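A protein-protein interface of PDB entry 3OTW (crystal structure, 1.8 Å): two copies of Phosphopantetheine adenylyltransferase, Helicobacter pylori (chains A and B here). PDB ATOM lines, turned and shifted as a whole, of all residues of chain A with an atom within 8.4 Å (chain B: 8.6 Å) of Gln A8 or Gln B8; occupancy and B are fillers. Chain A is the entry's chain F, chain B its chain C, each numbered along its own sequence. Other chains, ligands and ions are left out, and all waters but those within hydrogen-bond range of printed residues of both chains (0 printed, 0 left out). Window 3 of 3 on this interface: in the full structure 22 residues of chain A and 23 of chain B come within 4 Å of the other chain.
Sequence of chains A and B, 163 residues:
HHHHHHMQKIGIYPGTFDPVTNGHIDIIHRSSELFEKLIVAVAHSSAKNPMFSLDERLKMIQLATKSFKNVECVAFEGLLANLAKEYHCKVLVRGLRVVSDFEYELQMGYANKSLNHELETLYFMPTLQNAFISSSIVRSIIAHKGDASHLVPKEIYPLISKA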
ATOM      1  N   MET A   7      29.052 -11.457 -23.436  1.00  0.00           N
ATOM      2  CA  MET A   7      27.978 -11.255 -22.403  1.00  0.00           C
ATOM      3  C   MET A   7      26.760 -10.572 -23.043  1.00  0.00           C
ATOM      4  O   MET A   7      25.608 -10.905 -22.752  1.00  0.00           O
ATOM      5  CB  MET A   7      28.523 -10.421 -21.231  1.00  0.00           C
ATOM      6  CG  MET A   7      27.566 -10.256 -20.077  1.00  0.00           C
ATOM      7  SD  MET A   7      28.319  -9.458 -18.641  1.00  0.00           S
ATOM      8  CE  MET A   7      26.855  -9.060 -17.688  1.00  0.00           C
ATOM      9  N   GLN A   8      27.059  -9.619 -23.916  1.00  0.00           N
ATOM     10  CA  GLN A   8      26.112  -8.917 -24.794  1.00  0.00           C
ATOM     11  C   GLN A   8      25.324  -9.817 -25.758  1.00  0.00           C
ATOM     12  O   GLN A   8      24.223  -9.452 -26.174  1.00  0.00           O
ATOM     13  CB  GLN A   8      26.917  -7.866 -25.602  1.00  0.00           C
ATOM     14  CG  GLN A   8      26.383  -7.425 -26.998  1.00  0.00           C
ATOM     15  CD  GLN A   8      25.178  -6.518 -26.862  1.00  0.00           C
ATOM     16  OE1 GLN A   8      24.910  -6.011 -25.771  1.00  0.00           O
ATOM     17  NE2 GLN A   8      24.435  -6.319 -27.952  1.00  0.00           N
ATOM     18  N   LYS A   9      25.892 -10.972 -26.106  1.00  0.00           N
ATOM     19  CA  LYS A   9      25.392 -11.806 -27.211  1.00  0.00           C
ATOM     20  C   LYS A   9      23.984 -12.344 -27.007  1.00  0.00           C
ATOM     21  O   LYS A   9      23.182 -12.440 -27.950  1.00  0.00           O
ATOM     22  CB  LYS A   9      26.331 -13.005 -27.451  1.00  0.00           C
ATOM     23  CG  LYS A   9      27.470 -12.747 -28.427  1.00  0.00           C
ATOM     24  CD  LYS A   9      28.289 -14.033 -28.620  1.00  0.00           C
ATOM     25  CE  LYS A   9      29.400 -13.875 -29.643  1.00  0.00           C
ATOM     26  NZ  LYS A   9      30.569 -13.112 -29.118  1.00  0.00           N
ATOM     27  N   ILE A  10      23.683 -12.723 -25.773  1.00  0.00           N
ATOM     28  CA  ILE A  10      22.488 -13.486 -25.529  1.00  0.00           C
ATOM     29  C   ILE A  10      22.113 -13.349 -24.069  1.00  0.00           C
ATOM     30  O   ILE A  10      22.975 -13.378 -23.188  1.00  0.00           O
ATOM     31  CB  ILE A  10      22.681 -14.975 -25.923  1.00  0.00           C
ATOM     32  CG1 ILE A  10      21.404 -15.793 -25.698  1.00  0.00           C
ATOM     33  CG2 ILE A  10      23.912 -15.598 -25.216  1.00  0.00           C
ATOM     34  CD1 ILE A  10      21.317 -16.974 -26.689  1.00  0.00           C
ATOM     35  N   GLY A  11      20.830 -13.133 -23.848  1.00  0.00           N
ATOM     36  CA  GLY A  11      20.268 -13.184 -22.508  1.00  0.00           C
ATOM     37  C   GLY A  11      19.068 -14.096 -22.504  1.00  0.00           C
ATOM     38  O   GLY A  11      18.392 -14.228 -23.513  1.00  0.00           O
ATOM     39  N   ARG A  30      12.733  -3.887 -23.173  1.00  0.00           N
ATOM     40  CA  ARG A  30      13.984  -3.298 -22.700  1.00  0.00           C
ATOM     41  C   ARG A  30      15.182  -4.208 -22.828  1.00  0.00           C
ATOM     42  O   ARG A  30      16.258  -3.771 -23.268  1.00  0.00           O
ATOM     43  CB  ARG A  30      13.821  -2.875 -21.241  1.00  0.00           C
ATOM     44  CG  ARG A  30      13.214  -1.500 -21.163  1.00  0.00           C
ATOM     45  CD  ARG A  30      12.196  -1.326 -20.048  1.00  0.00           C
ATOM     46  NE  ARG A  30      11.472  -0.073 -20.304  1.00  0.00           N
ATOM     47  CZ  ARG A  30      10.360   0.036 -21.033  1.00  0.00           C
ATOM     48  NH1 ARG A  30       9.817   1.231 -21.221  1.00  0.00           N
ATOM     49  NH2 ARG A  30       9.779  -1.038 -21.564  1.00  0.00           N
ATOM     50  N   SER A  31      15.009  -5.466 -22.421  1.00  0.00           N
ATOM     51  CA  SER A  31      16.124  -6.388 -22.446  1.00  0.00           C
ATOM     52  C   SER A  31      16.500  -6.780 -23.889  1.00  0.00           C
ATOM     53  O   SER A  31      17.670  -6.973 -24.167  1.00  0.00           O
ATOM     54  CB  SER A  31      15.864  -7.613 -21.540  1.00  0.00           C
ATOM     55  OG  SER A  31      14.798  -8.402 -22.031  1.00  0.00           O
ATOM     56  N   SER A  32      15.508  -6.853 -24.778  1.00  0.00           N
ATOM     57  CA  SER A  32      15.753  -7.179 -26.212  1.00  0.00           C
ATOM     58  C   SER A  32      16.461  -6.039 -26.947  1.00  0.00           C
ATOM     59  O   SER A  32      17.074  -6.240 -28.019  1.00  0.00           O
ATOM     60  CB  SER A  32      14.450  -7.559 -26.920  1.00  0.00           C
ATOM     61  OG  SER A  32      13.639  -6.419 -27.159  1.00  0.00           O
ATOM     62  N   GLU A  33      16.396  -4.842 -26.368  1.00  0.00           N
ATOM     63  CA  GLU A  33      17.170  -3.715 -26.865  1.00  0.00           C
ATOM     64  C   GLU A  33      18.623  -3.890 -26.496  1.00  0.00           C
ATOM     65  O   GLU A  33      19.507  -3.489 -27.236  1.00  0.00           O
ATOM     66  CB  GLU A  33      16.704  -2.413 -26.242  1.00  0.00           C
ATOM     67  CG  GLU A  33      15.381  -1.888 -26.686  1.00  0.00           C
ATOM     68  CD  GLU A  33      15.299  -0.382 -26.501  1.00  0.00           C
ATOM     69  OE1 GLU A  33      14.171   0.168 -26.574  1.00  0.00           O
ATOM     70  OE2 GLU A  33      16.368   0.257 -26.300  1.00  0.00           O
ATOM     71  N   LEU A  34      18.875  -4.484 -25.335  1.00  0.00           N
ATOM     72  CA  LEU A  34      20.229  -4.619 -24.842  1.00  0.00           C
ATOM     73  C   LEU A  34      21.005  -5.754 -25.494  1.00  0.00           C
ATOM     74  O   LEU A  34      22.126  -5.549 -25.950  1.00  0.00           O
ATOM     75  CB  LEU A  34      20.242  -4.762 -23.317  1.00  0.00           C
ATOM     76  CG  LEU A  34      21.612  -4.770 -22.627  1.00  0.00           C
ATOM     77  CD1 LEU A  34      22.374  -3.463 -22.800  1.00  0.00           C
ATOM     78  CD2 LEU A  34      21.402  -5.070 -21.155  1.00  0.00           C
ATOM     79  N   PHE A  35      20.404  -6.932 -25.565  1.00  0.00           N
ATOM     80  CA  PHE A  35      21.103  -8.117 -26.044  1.00  0.00           C
ATOM     81  C   PHE A  35      20.908  -8.334 -27.536  1.00  0.00           C
ATOM     82  O   PHE A  35      19.858  -8.007 -28.092  1.00  0.00           O
ATOM     83  CB  PHE A  35      20.581  -9.346 -25.309  1.00  0.00           C
ATOM     84  CG  PHE A  35      20.867  -9.317 -23.847  1.00  0.00           C
ATOM     85  CD1 PHE A  35      19.891  -8.931 -22.941  1.00  0.00           C
ATOM     86  CD2 PHE A  35      22.125  -9.678 -23.383  1.00  0.00           C
ATOM     87  CE1 PHE A  35      20.180  -8.884 -21.593  1.00  0.00           C
ATOM     88  CE2 PHE A  35      22.420  -9.633 -22.023  1.00  0.00           C
ATOM     89  CZ  PHE A  35      21.450  -9.238 -21.143  1.00  0.00           C
ATOM     90  N   GLU A  36      21.912  -8.929 -28.164  1.00  0.00           N
ATOM     91  CA  GLU A  36      21.813  -9.252 -29.585  1.00  0.00           C
ATOM     92  C   GLU A  36      20.701 -10.255 -29.854  1.00  0.00           C
ATOM     93  O   GLU A  36      19.977 -10.132 -30.846  1.00  0.00           O
ATOM     94  CB  GLU A  36      23.150  -9.750 -30.107  1.00  0.00           C
ATOM     95  CG  GLU A  36      24.118  -8.613 -30.339  1.00  0.00           C
ATOM     96  CD  GLU A  36      25.479  -9.062 -30.825  1.00  0.00           C
ATOM     97  OE1 GLU A  36      25.579 -10.092 -31.548  1.00  0.00           O
ATOM     98  OE2 GLU A  36      26.455  -8.349 -30.502  1.00  0.00           O
ATOM     99  N   LYS A  37      20.569 -11.238 -28.959  1.00  0.00           N
ATOM    100  CA  LYS A  37      19.472 -12.199 -28.974  1.00  0.00           C
ATOM    101  C   LYS A  37      18.853 -12.301 -27.589  1.00  0.00           C
ATOM    102  O   LYS A  37      19.575 -12.402 -26.605  1.00  0.00           O
ATOM    103  CB  LYS A  37      20.015 -13.568 -29.383  1.00  0.00           C
ATOM    104  CG  LYS A  37      19.040 -14.731 -29.275  1.00  0.00           C
ATOM    105  CD  LYS A  37      18.282 -15.006 -30.575  1.00  0.00           C
ATOM    106  CE  LYS A  37      18.145 -16.517 -30.764  1.00  0.00           C
ATOM    107  NZ  LYS A  37      16.943 -16.924 -31.537  1.00  0.00           N
ATOM    108  N   LEU A  38      17.528 -12.282 -27.494  1.00  0.00           N
ATOM    109  CA  LEU A  38      16.881 -12.601 -26.204  1.00  0.00           C
ATOM    110  C   LEU A  38      16.087 -13.890 -26.351  1.00  0.00           C
ATOM    111  O   LEU A  38      15.252 -14.008 -27.264  1.00  0.00           O
ATOM    112  CB  LEU A  38      15.966 -11.457 -25.751  1.00  0.00           C
ATOM    113  CG  LEU A  38      15.300 -11.625 -24.372  1.00  0.00           C
ATOM    114  CD1 LEU A  38      16.311 -11.354 -23.237  1.00  0.00           C
ATOM    115  CD2 LEU A  38      14.118 -10.700 -24.279  1.00  0.00           C
ATOM    116  N   ASN A  70      14.530 -10.034 -32.610  1.00  0.00           N
ATOM    117  CA  ASN A  70      15.673 -10.712 -32.011  1.00  0.00           C
ATOM    118  C   ASN A  70      15.285 -11.505 -30.758  1.00  0.00           C
ATOM    119  O   ASN A  70      16.151 -11.869 -29.956  1.00  0.00           O
ATOM    120  CB  ASN A  70      16.786  -9.711 -31.700  1.00  0.00           C
ATOM    121  CG  ASN A  70      16.435  -8.804 -30.532  1.00  0.00           C
ATOM    122  OD1 ASN A  70      15.266  -8.518 -30.289  1.00  0.00           O
ATOM    123  ND2 ASN A  70      17.450  -8.343 -29.815  1.00  0.00           N
ATOM    124  N   LYS A  90      25.450 -16.236 -20.488  1.00  0.00           N
ATOM    125  CA  LYS A  90      26.045 -15.859 -19.191  1.00  0.00           C
ATOM    126  C   LYS A  90      25.158 -14.915 -18.377  1.00  0.00           C
ATOM    127  O   LYS A  90      25.578 -14.464 -17.295  1.00  0.00           O
ATOM    128  CB  LYS A  90      27.432 -15.235 -19.399  1.00  0.00           C
ATOM    129  CG  LYS A  90      28.456 -16.272 -19.878  1.00  0.00           C
ATOM    130  CD  LYS A  90      29.459 -15.698 -20.870  1.00  0.00           C
ATOM    131  CE  LYS A  90      30.136 -16.791 -21.706  1.00  0.00           C
ATOM    132  NZ  LYS A  90      29.542 -17.044 -23.083  1.00  0.00           N
ATOM    133  N   VAL A  91      23.958 -14.602 -18.885  1.00  0.00           N
ATOM    134  CA  VAL A  91      23.076 -13.607 -18.228  1.00  0.00           C
ATOM    135  C   VAL A  91      21.637 -14.013 -18.236  1.00  0.00           C
ATOM    136  O   VAL A  91      21.053 -14.229 -19.310  1.00  0.00           O
ATOM    137  CB  VAL A  91      23.097 -12.195 -18.879  1.00  0.00           C
ATOM    138  CG1 VAL A  91      22.250 -11.171 -18.027  1.00  0.00           C
ATOM    139  CG2 VAL A  91      24.472 -11.714 -19.048  1.00  0.00           C
ATOM    140  N   MET B   7      22.211   1.421 -26.285  1.00  0.00           N
ATOM    141  CA  MET B   7      21.964   0.833 -24.945  1.00  0.00           C
ATOM    142  C   MET B   7      23.204   0.059 -24.536  1.00  0.00           C
ATOM    143  O   MET B   7      23.743   0.273 -23.451  1.00  0.00           O
ATOM    144  CB  MET B   7      20.716  -0.063 -24.966  1.00  0.00           C
ATOM    145  CG  MET B   7      20.190  -0.421 -23.613  1.00  0.00           C
ATOM    146  SD  MET B   7      18.436  -0.882 -23.591  1.00  0.00           S
ATOM    147  CE  MET B   7      18.263  -1.413 -21.895  1.00  0.00           C
ATOM    148  N   GLN B   8      23.684  -0.815 -25.413  1.00  0.00           N
ATOM    149  CA  GLN B   8      24.854  -1.621 -25.084  1.00  0.00           C
ATOM    150  C   GLN B   8      26.159  -0.807 -25.147  1.00  0.00           C
ATOM    151  O   GLN B   8      27.166  -1.209 -24.575  1.00  0.00           O
ATOM    152  CB  GLN B   8      24.908  -2.875 -25.971  1.00  0.00           C
ATOM    153  CG  GLN B   8      25.994  -2.890 -27.085  1.00  0.00           C
ATOM    154  CD  GLN B   8      27.310  -3.502 -26.583  1.00  0.00           C
ATOM    155  OE1 GLN B   8      27.370  -4.091 -25.486  1.00  0.00           O
ATOM    156  NE2 GLN B   8      28.355  -3.371 -27.375  1.00  0.00           N
ATOM    157  N   LYS B   9      26.127   0.351 -25.815  1.00  0.00           N
ATOM    158  CA  LYS B   9      27.352   1.137 -25.997  1.00  0.00           C
ATOM    159  C   LYS B   9      27.967   1.738 -24.722  1.00  0.00           C
ATOM    160  O   LYS B   9      29.199   1.827 -24.575  1.00  0.00           O
ATOM    161  CB  LYS B   9      27.135   2.248 -27.013  1.00  0.00           C
ATOM    162  CG  LYS B   9      28.438   2.898 -27.429  1.00  0.00           C
ATOM    163  CD  LYS B   9      28.304   3.776 -28.670  1.00  0.00           C
ATOM    164  CE  LYS B   9      29.308   4.931 -28.570  1.00  0.00           C
ATOM    165  NZ  LYS B   9      28.962   5.874 -27.413  1.00  0.00           N
ATOM    166  N   ILE B  10      27.116   2.148 -23.799  1.00  0.00           N
ATOM    167  CA  ILE B  10      27.623   2.869 -22.646  1.00  0.00           C
ATOM    168  C   ILE B  10      26.659   2.755 -21.502  1.00  0.00           C
ATOM    169  O   ILE B  10      25.432   2.853 -21.679  1.00  0.00           O
ATOM    170  CB  ILE B  10      27.894   4.370 -22.981  1.00  0.00           C
ATOM    171  CG1 ILE B  10      28.549   5.112 -21.809  1.00  0.00           C
ATOM    172  CG2 ILE B  10      26.615   5.081 -23.460  1.00  0.00           C
ATOM    173  CD1 ILE B  10      29.335   6.395 -22.310  1.00  0.00           C
ATOM    174  N   GLY B  11      27.215   2.517 -20.321  1.00  0.00           N
ATOM    175  CA  GLY B  11      26.408   2.620 -19.108  1.00  0.00           C
ATOM    176  C   GLY B  11      27.093   3.566 -18.126  1.00  0.00           C
ATOM    177  O   GLY B  11      28.320   3.741 -18.221  1.00  0.00           O
ATOM    178  N   SER B  31      29.289  -4.949 -14.674  1.00  0.00           N
ATOM    179  CA  SER B  31      28.693  -4.053 -15.665  1.00  0.00           C
ATOM    180  C   SER B  31      29.679  -3.712 -16.790  1.00  0.00           C
ATOM    181  O   SER B  31      29.267  -3.532 -17.940  1.00  0.00           O
ATOM    182  CB  SER B  31      28.130  -2.786 -15.014  1.00  0.00           C
ATOM    183  OG  SER B  31      29.136  -2.039 -14.373  1.00  0.00           O
ATOM    184  N   SER B  32      30.976  -3.657 -16.483  1.00  0.00           N
ATOM    185  CA  SER B  32      31.981  -3.370 -17.523  1.00  0.00           C
ATOM    186  C   SER B  32      32.144  -4.519 -18.515  1.00  0.00           C
ATOM    187  O   SER B  32      32.590  -4.287 -19.636  1.00  0.00           O
ATOM    188  CB  SER B  32      33.342  -3.020 -16.924  1.00  0.00           C
ATOM    189  OG  SER B  32      33.952  -4.152 -16.324  1.00  0.00           O
ATOM    190  N   GLU B  33      31.794  -5.745 -18.108  1.00  0.00           N
ATOM    191  CA  GLU B  33      31.778  -6.886 -19.028  1.00  0.00           C
ATOM    192  C   GLU B  33      30.607  -6.814 -19.984  1.00  0.00           C
ATOM    193  O   GLU B  33      30.630  -7.455 -21.043  1.00  0.00           O
ATOM    194  CB  GLU B  33      31.700  -8.215 -18.287  1.00  0.00           C
ATOM    195  CG  GLU B  33      32.955  -8.616 -17.565  1.00  0.00           C
ATOM    196  CD  GLU B  33      32.741  -9.890 -16.780  1.00  0.00           C
ATOM    197  OE1 GLU B  33      33.199  -9.971 -15.623  1.00  0.00           O
ATOM    198  OE2 GLU B  33      32.071 -10.800 -17.309  1.00  0.00           O
ATOM    199  N   LEU B  34      29.591  -6.045 -19.619  1.00  0.00           N
ATOM    200  CA  LEU B  34      28.404  -5.928 -20.453  1.00  0.00           C
ATOM    201  C   LEU B  34      28.434  -4.781 -21.481  1.00  0.00           C
ATOM    202  O   LEU B  34      28.162  -5.027 -22.679  1.00  0.00           O
ATOM    203  CB  LEU B  34      27.149  -5.884 -19.588  1.00  0.00           C
ATOM    204  CG  LEU B  34      25.802  -5.946 -20.292  1.00  0.00           C
ATOM    205  CD1 LEU B  34      25.582  -7.289 -21.008  1.00  0.00           C
ATOM    206  CD2 LEU B  34      24.735  -5.728 -19.220  1.00  0.00           C
ATOM    207  N   PHE B  35      28.789  -3.567 -21.035  1.00  0.00           N
ATOM    208  CA  PHE B  35      28.813  -2.362 -21.877  1.00  0.00           C
ATOM    209  C   PHE B  35      30.143  -2.141 -22.576  1.00  0.00           C
ATOM    210  O   PHE B  35      31.186  -2.446 -22.023  1.00  0.00           O
ATOM    211  CB  PHE B  35      28.503  -1.109 -21.033  1.00  0.00           C
ATOM    212  CG  PHE B  35      27.160  -1.144 -20.406  1.00  0.00           C
ATOM    213  CD1 PHE B  35      27.008  -1.551 -19.082  1.00  0.00           C
ATOM    214  CD2 PHE B  35      26.025  -0.813 -21.143  1.00  0.00           C
ATOM    215  CE1 PHE B  35      25.747  -1.642 -18.509  1.00  0.00           C
ATOM    216  CE2 PHE B  35      24.766  -0.888 -20.563  1.00  0.00           C
ATOM    217  CZ  PHE B  35      24.635  -1.301 -19.234  1.00  0.00           C
ATOM    218  N   GLU B  36      30.101  -1.584 -23.779  1.00  0.00           N
ATOM    219  CA  GLU B  36      31.350  -1.247 -24.481  1.00  0.00           C
ATOM    220  C   GLU B  36      32.202  -0.277 -23.631  1.00  0.00           C
ATOM    221  O   GLU B  36      33.421  -0.450 -23.510  1.00  0.00           O
ATOM    222  CB  GLU B  36      31.078  -0.703 -25.890  1.00  0.00           C
ATOM    223  CG  GLU B  36      32.353  -0.597 -26.724  1.00  0.00           C
ATOM    224  CD  GLU B  36      32.226   0.376 -27.893  1.00  0.00           C
ATOM    225  OE1 GLU B  36      31.188   0.325 -28.597  1.00  0.00           O
ATOM    226  OE2 GLU B  36      33.170   1.181 -28.109  1.00  0.00           O
ATOM    227  N   LYS B  37      31.537   0.700 -23.008  1.00  0.00           N
ATOM    228  CA  LYS B  37      32.174   1.629 -22.094  1.00  0.00           C
ATOM    229  C   LYS B  37      31.340   1.768 -20.832  1.00  0.00           C
ATOM    230  O   LYS B  37      30.116   1.851 -20.890  1.00  0.00           O
ATOM    231  CB  LYS B  37      32.312   3.014 -22.728  1.00  0.00           C
ATOM    232  CG  LYS B  37      33.301   3.895 -21.999  1.00  0.00           C
ATOM    233  CD  LYS B  37      33.480   5.272 -22.689  1.00  0.00           C
ATOM    234  CE  LYS B  37      33.867   5.171 -24.147  1.00  0.00           C
ATOM    235  NZ  LYS B  37      34.439   6.467 -24.645  1.00  0.00           N
ATOM    236  N   LEU B  38      32.023   1.801 -19.692  1.00  0.00           N
ATOM    237  CA  LEU B  38      31.338   2.068 -18.442  1.00  0.00           C
ATOM    238  C   LEU B  38      31.925   3.330 -17.833  1.00  0.00           C
ATOM    239  O   LEU B  38      33.141   3.468 -17.674  1.00  0.00           O
ATOM    240  CB  LEU B  38      31.480   0.903 -17.475  1.00  0.00           C
ATOM    241  CG  LEU B  38      30.745   1.165 -16.150  1.00  0.00           C
ATOM    242  CD1 LEU B  38      29.238   0.915 -16.340  1.00  0.00           C
ATOM    243  CD2 LEU B  38      31.386   0.323 -15.020  1.00  0.00           C
ATOM    244  N   ASN B  70      38.074  -0.546 -20.025  1.00  0.00           N
ATOM    245  CA  ASN B  70      36.950   0.169 -20.616  1.00  0.00           C
ATOM    246  C   ASN B  70      36.143   0.962 -19.576  1.00  0.00           C
ATOM    247  O   ASN B  70      35.009   1.333 -19.841  1.00  0.00           O
ATOM    248  CB  ASN B  70      36.028  -0.785 -21.406  1.00  0.00           C
ATOM    249  CG  ASN B  70      35.209  -1.704 -20.485  1.00  0.00           C
ATOM    250  OD1 ASN B  70      35.676  -2.081 -19.399  1.00  0.00           O
ATOM    251  ND2 ASN B  70      33.988  -2.055 -20.915  1.00  0.00           N
ATOM    252  N   HIS B  88      25.328  10.524 -24.235  1.00  0.00           N
ATOM    253  CA  HIS B  88      24.339   9.830 -25.055  1.00  0.00           C
ATOM    254  C   HIS B  88      24.092   8.429 -24.477  1.00  0.00           C
ATOM    255  O   HIS B  88      23.986   7.443 -25.205  1.00  0.00           O
ATOM    256  CB  HIS B  88      24.778   9.764 -26.545  1.00  0.00           C
ATOM    257  CG  HIS B  88      23.653   9.459 -27.472  1.00  0.00           C
ATOM    258  ND1 HIS B  88      22.537  10.267 -27.576  1.00  0.00           N
ATOM    259  CD2 HIS B  88      23.463   8.438 -28.340  1.00  0.00           C
ATOM    260  CE1 HIS B  88      21.708   9.749 -28.469  1.00  0.00           C
ATOM    261  NE2 HIS B  88      22.245   8.638 -28.942  1.00  0.00           N
ATOM    262  N   CYS B  89      23.987   8.405 -23.153  1.00  0.00           N
ATOM    263  CA  CYS B  89      23.840   7.176 -22.375  1.00  0.00           C
ATOM    264  C   CYS B  89      22.366   7.001 -21.999  1.00  0.00           C
ATOM    265  O   CYS B  89      21.738   7.920 -21.466  1.00  0.00           O
ATOM    266  CB  CYS B  89      24.681   7.318 -21.108  1.00  0.00           C
ATOM    267  SG  CYS B  89      24.475   5.844 -20.040  1.00  0.00           S
ATOM    268  N   LYS B  90      21.843   5.822 -22.287  1.00  0.00           N
ATOM    269  CA  LYS B  90      20.474   5.439 -21.982  1.00  0.00           C
ATOM    270  C   LYS B  90      20.330   4.473 -20.806  1.00  0.00           C
ATOM    271  O   LYS B  90      19.213   3.947 -20.587  1.00  0.00           O
ATOM    272  CB  LYS B  90      19.949   4.688 -23.200  1.00  0.00           C
ATOM    273  CG  LYS B  90      18.496   4.486 -23.222  1.00  0.00           C
ATOM    274  CD  LYS B  90      18.027   3.833 -24.532  1.00  0.00           C
ATOM    275  CE  LYS B  90      16.681   3.170 -24.286  1.00  0.00           C
ATOM    276  NZ  LYS B  90      15.760   4.078 -23.502  1.00  0.00           N
ATOM    277  N   VAL B  91      21.415   4.188 -20.095  1.00  0.00           N
ATOM    278  CA  VAL B  91      21.379   3.157 -19.035  1.00  0.00           C
ATOM    279  C   VAL B  91      22.179   3.590 -17.836  1.00  0.00           C
ATOM    280  O   VAL B  91      23.389   3.850 -17.947  1.00  0.00           O
ATOM    281  CB  VAL B  91      21.990   1.805 -19.510  1.00  0.00           C
ATOM    282  CG1 VAL B  91      21.840   0.771 -18.414  1.00  0.00           C
ATOM    283  CG2 VAL B  91      21.347   1.302 -20.797  1.00  0.00           C
ATOM    284  N   LEU B 122      19.308  -0.276 -14.827  1.00  0.00           N
ATOM    285  CA  LEU B 122      19.535  -1.738 -14.828  1.00  0.00           C
ATOM    286  C   LEU B 122      20.293  -2.092 -13.552  1.00  0.00           C
ATOM    287  O   LEU B 122      21.178  -1.324 -13.154  1.00  0.00           O
ATOM    288  CB  LEU B 122      20.451  -2.108 -16.019  1.00  0.00           C
ATOM    289  CG  LEU B 122      19.794  -2.413 -17.370  1.00  0.00           C
ATOM    290  CD1 LEU B 122      18.764  -1.355 -17.829  1.00  0.00           C
ATOM    291  CD2 LEU B 122      20.851  -2.612 -18.429  1.00  0.00           C
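The side-chain amide oxygen (OE1) of Gln B8 sits close to the side-chain amide oxygen (OE1) of Gln A8 (3.1 Å).
The side-chain sulfur (SD) of Met A7 is in hydrogen-bond range of the backbone NH (N) of Leu B34, 3.8 Å away.
The side-chain sulfur of Met B7 lies close to the backbone carbonyl oxygen of Arg A30 (3.6 Å).
The side-chain carboxylate (OE2) of Glu A33 sits close to the side-chain sulfur (SD) of Met B7 (3.6 Å).
The backbone carbonyl oxygen (O) of Leu B34 sits close to the side-chain amide oxygen (OE1) of Gln B8.
The backbone NH of Glu B36 sits at hydrogen-bond distance from the backbone carbonyl oxygen of Gln B8 (3.1 Å).
The backbone carbonyl oxygen of Leu A34 sits close to the side-chain amide oxygen of Gln A8, 2.8 Å away.
The backbone carbonyl oxygen (O) of Gln A8 lies within hydrogen-bond range of the backbone NH (N) of Glu A36 (3.1 Å).
Glu B33 touches Met A7 (CB to SD, 3.6 Å).
Lys B90 touches Glu A33.
CG of Met B7 touches CD1 of Leu A34, at 3.8 Å.
CD1 of Leu A34 touches CA of Gln B8, at 3.8 Å.
Leu B34 touches Leu A34.
Leu A34 touches Leu B122.
Of the printed residues of chain B, Gln A8 touches Gln B8.
Printed residues of chain A within 4 Å of Met B7: Arg A30 (3.4 Å), Glu A33 (3.5 Å) and Leu A34 (3.8 Å).
Of chain A, only Gln A8 and Leu A34 come within 4 Å of Gln B8.
Of the printed residues of chain A, Leu B122 touches Leu A34 (3.7 Å).
The nearest residue of chain A that does not touch Gln B8 is Glu A33 (5.3 Å).
The nearest printed residue of chain B that does not touch Glu A33 is Gln B8 (5.3 Å).
Printed residues of chain B that touch a printed residue of chain A: Met B7, Gln B8, Glu B33, Leu B34, Lys B90 and Leu B122.
Printed residues of chain A that touch a printed residue of chain B: Met A7, Gln A8, Arg A30, Glu A33 and Leu A34.
Hydrophobic or aromatic side chains of chain A within 4 Å of the printed part of chain B: Met A7 and Leu A34.
Met A7 touches Leu B34, and with the chains exchanged Leu A34 touches Met B7.
Gln A8 touches its own counterpart, Gln B8.
Leu A34 touches Gln B8, but with the chains exchanged Gln A8 does not touch Leu B34 (4.01 Å).
Leu B34 touches its own counterpart, Leu A34.
Positions printed for both chains: 7, 8, 9, 10, 11, 31, 32, 33, 34, 35, 36, 37, 38, 70, 90 and 91.
Of the 10 pairs that touch across the chains among the printed residues, 6 have their exchanged pair printed and touching as well.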
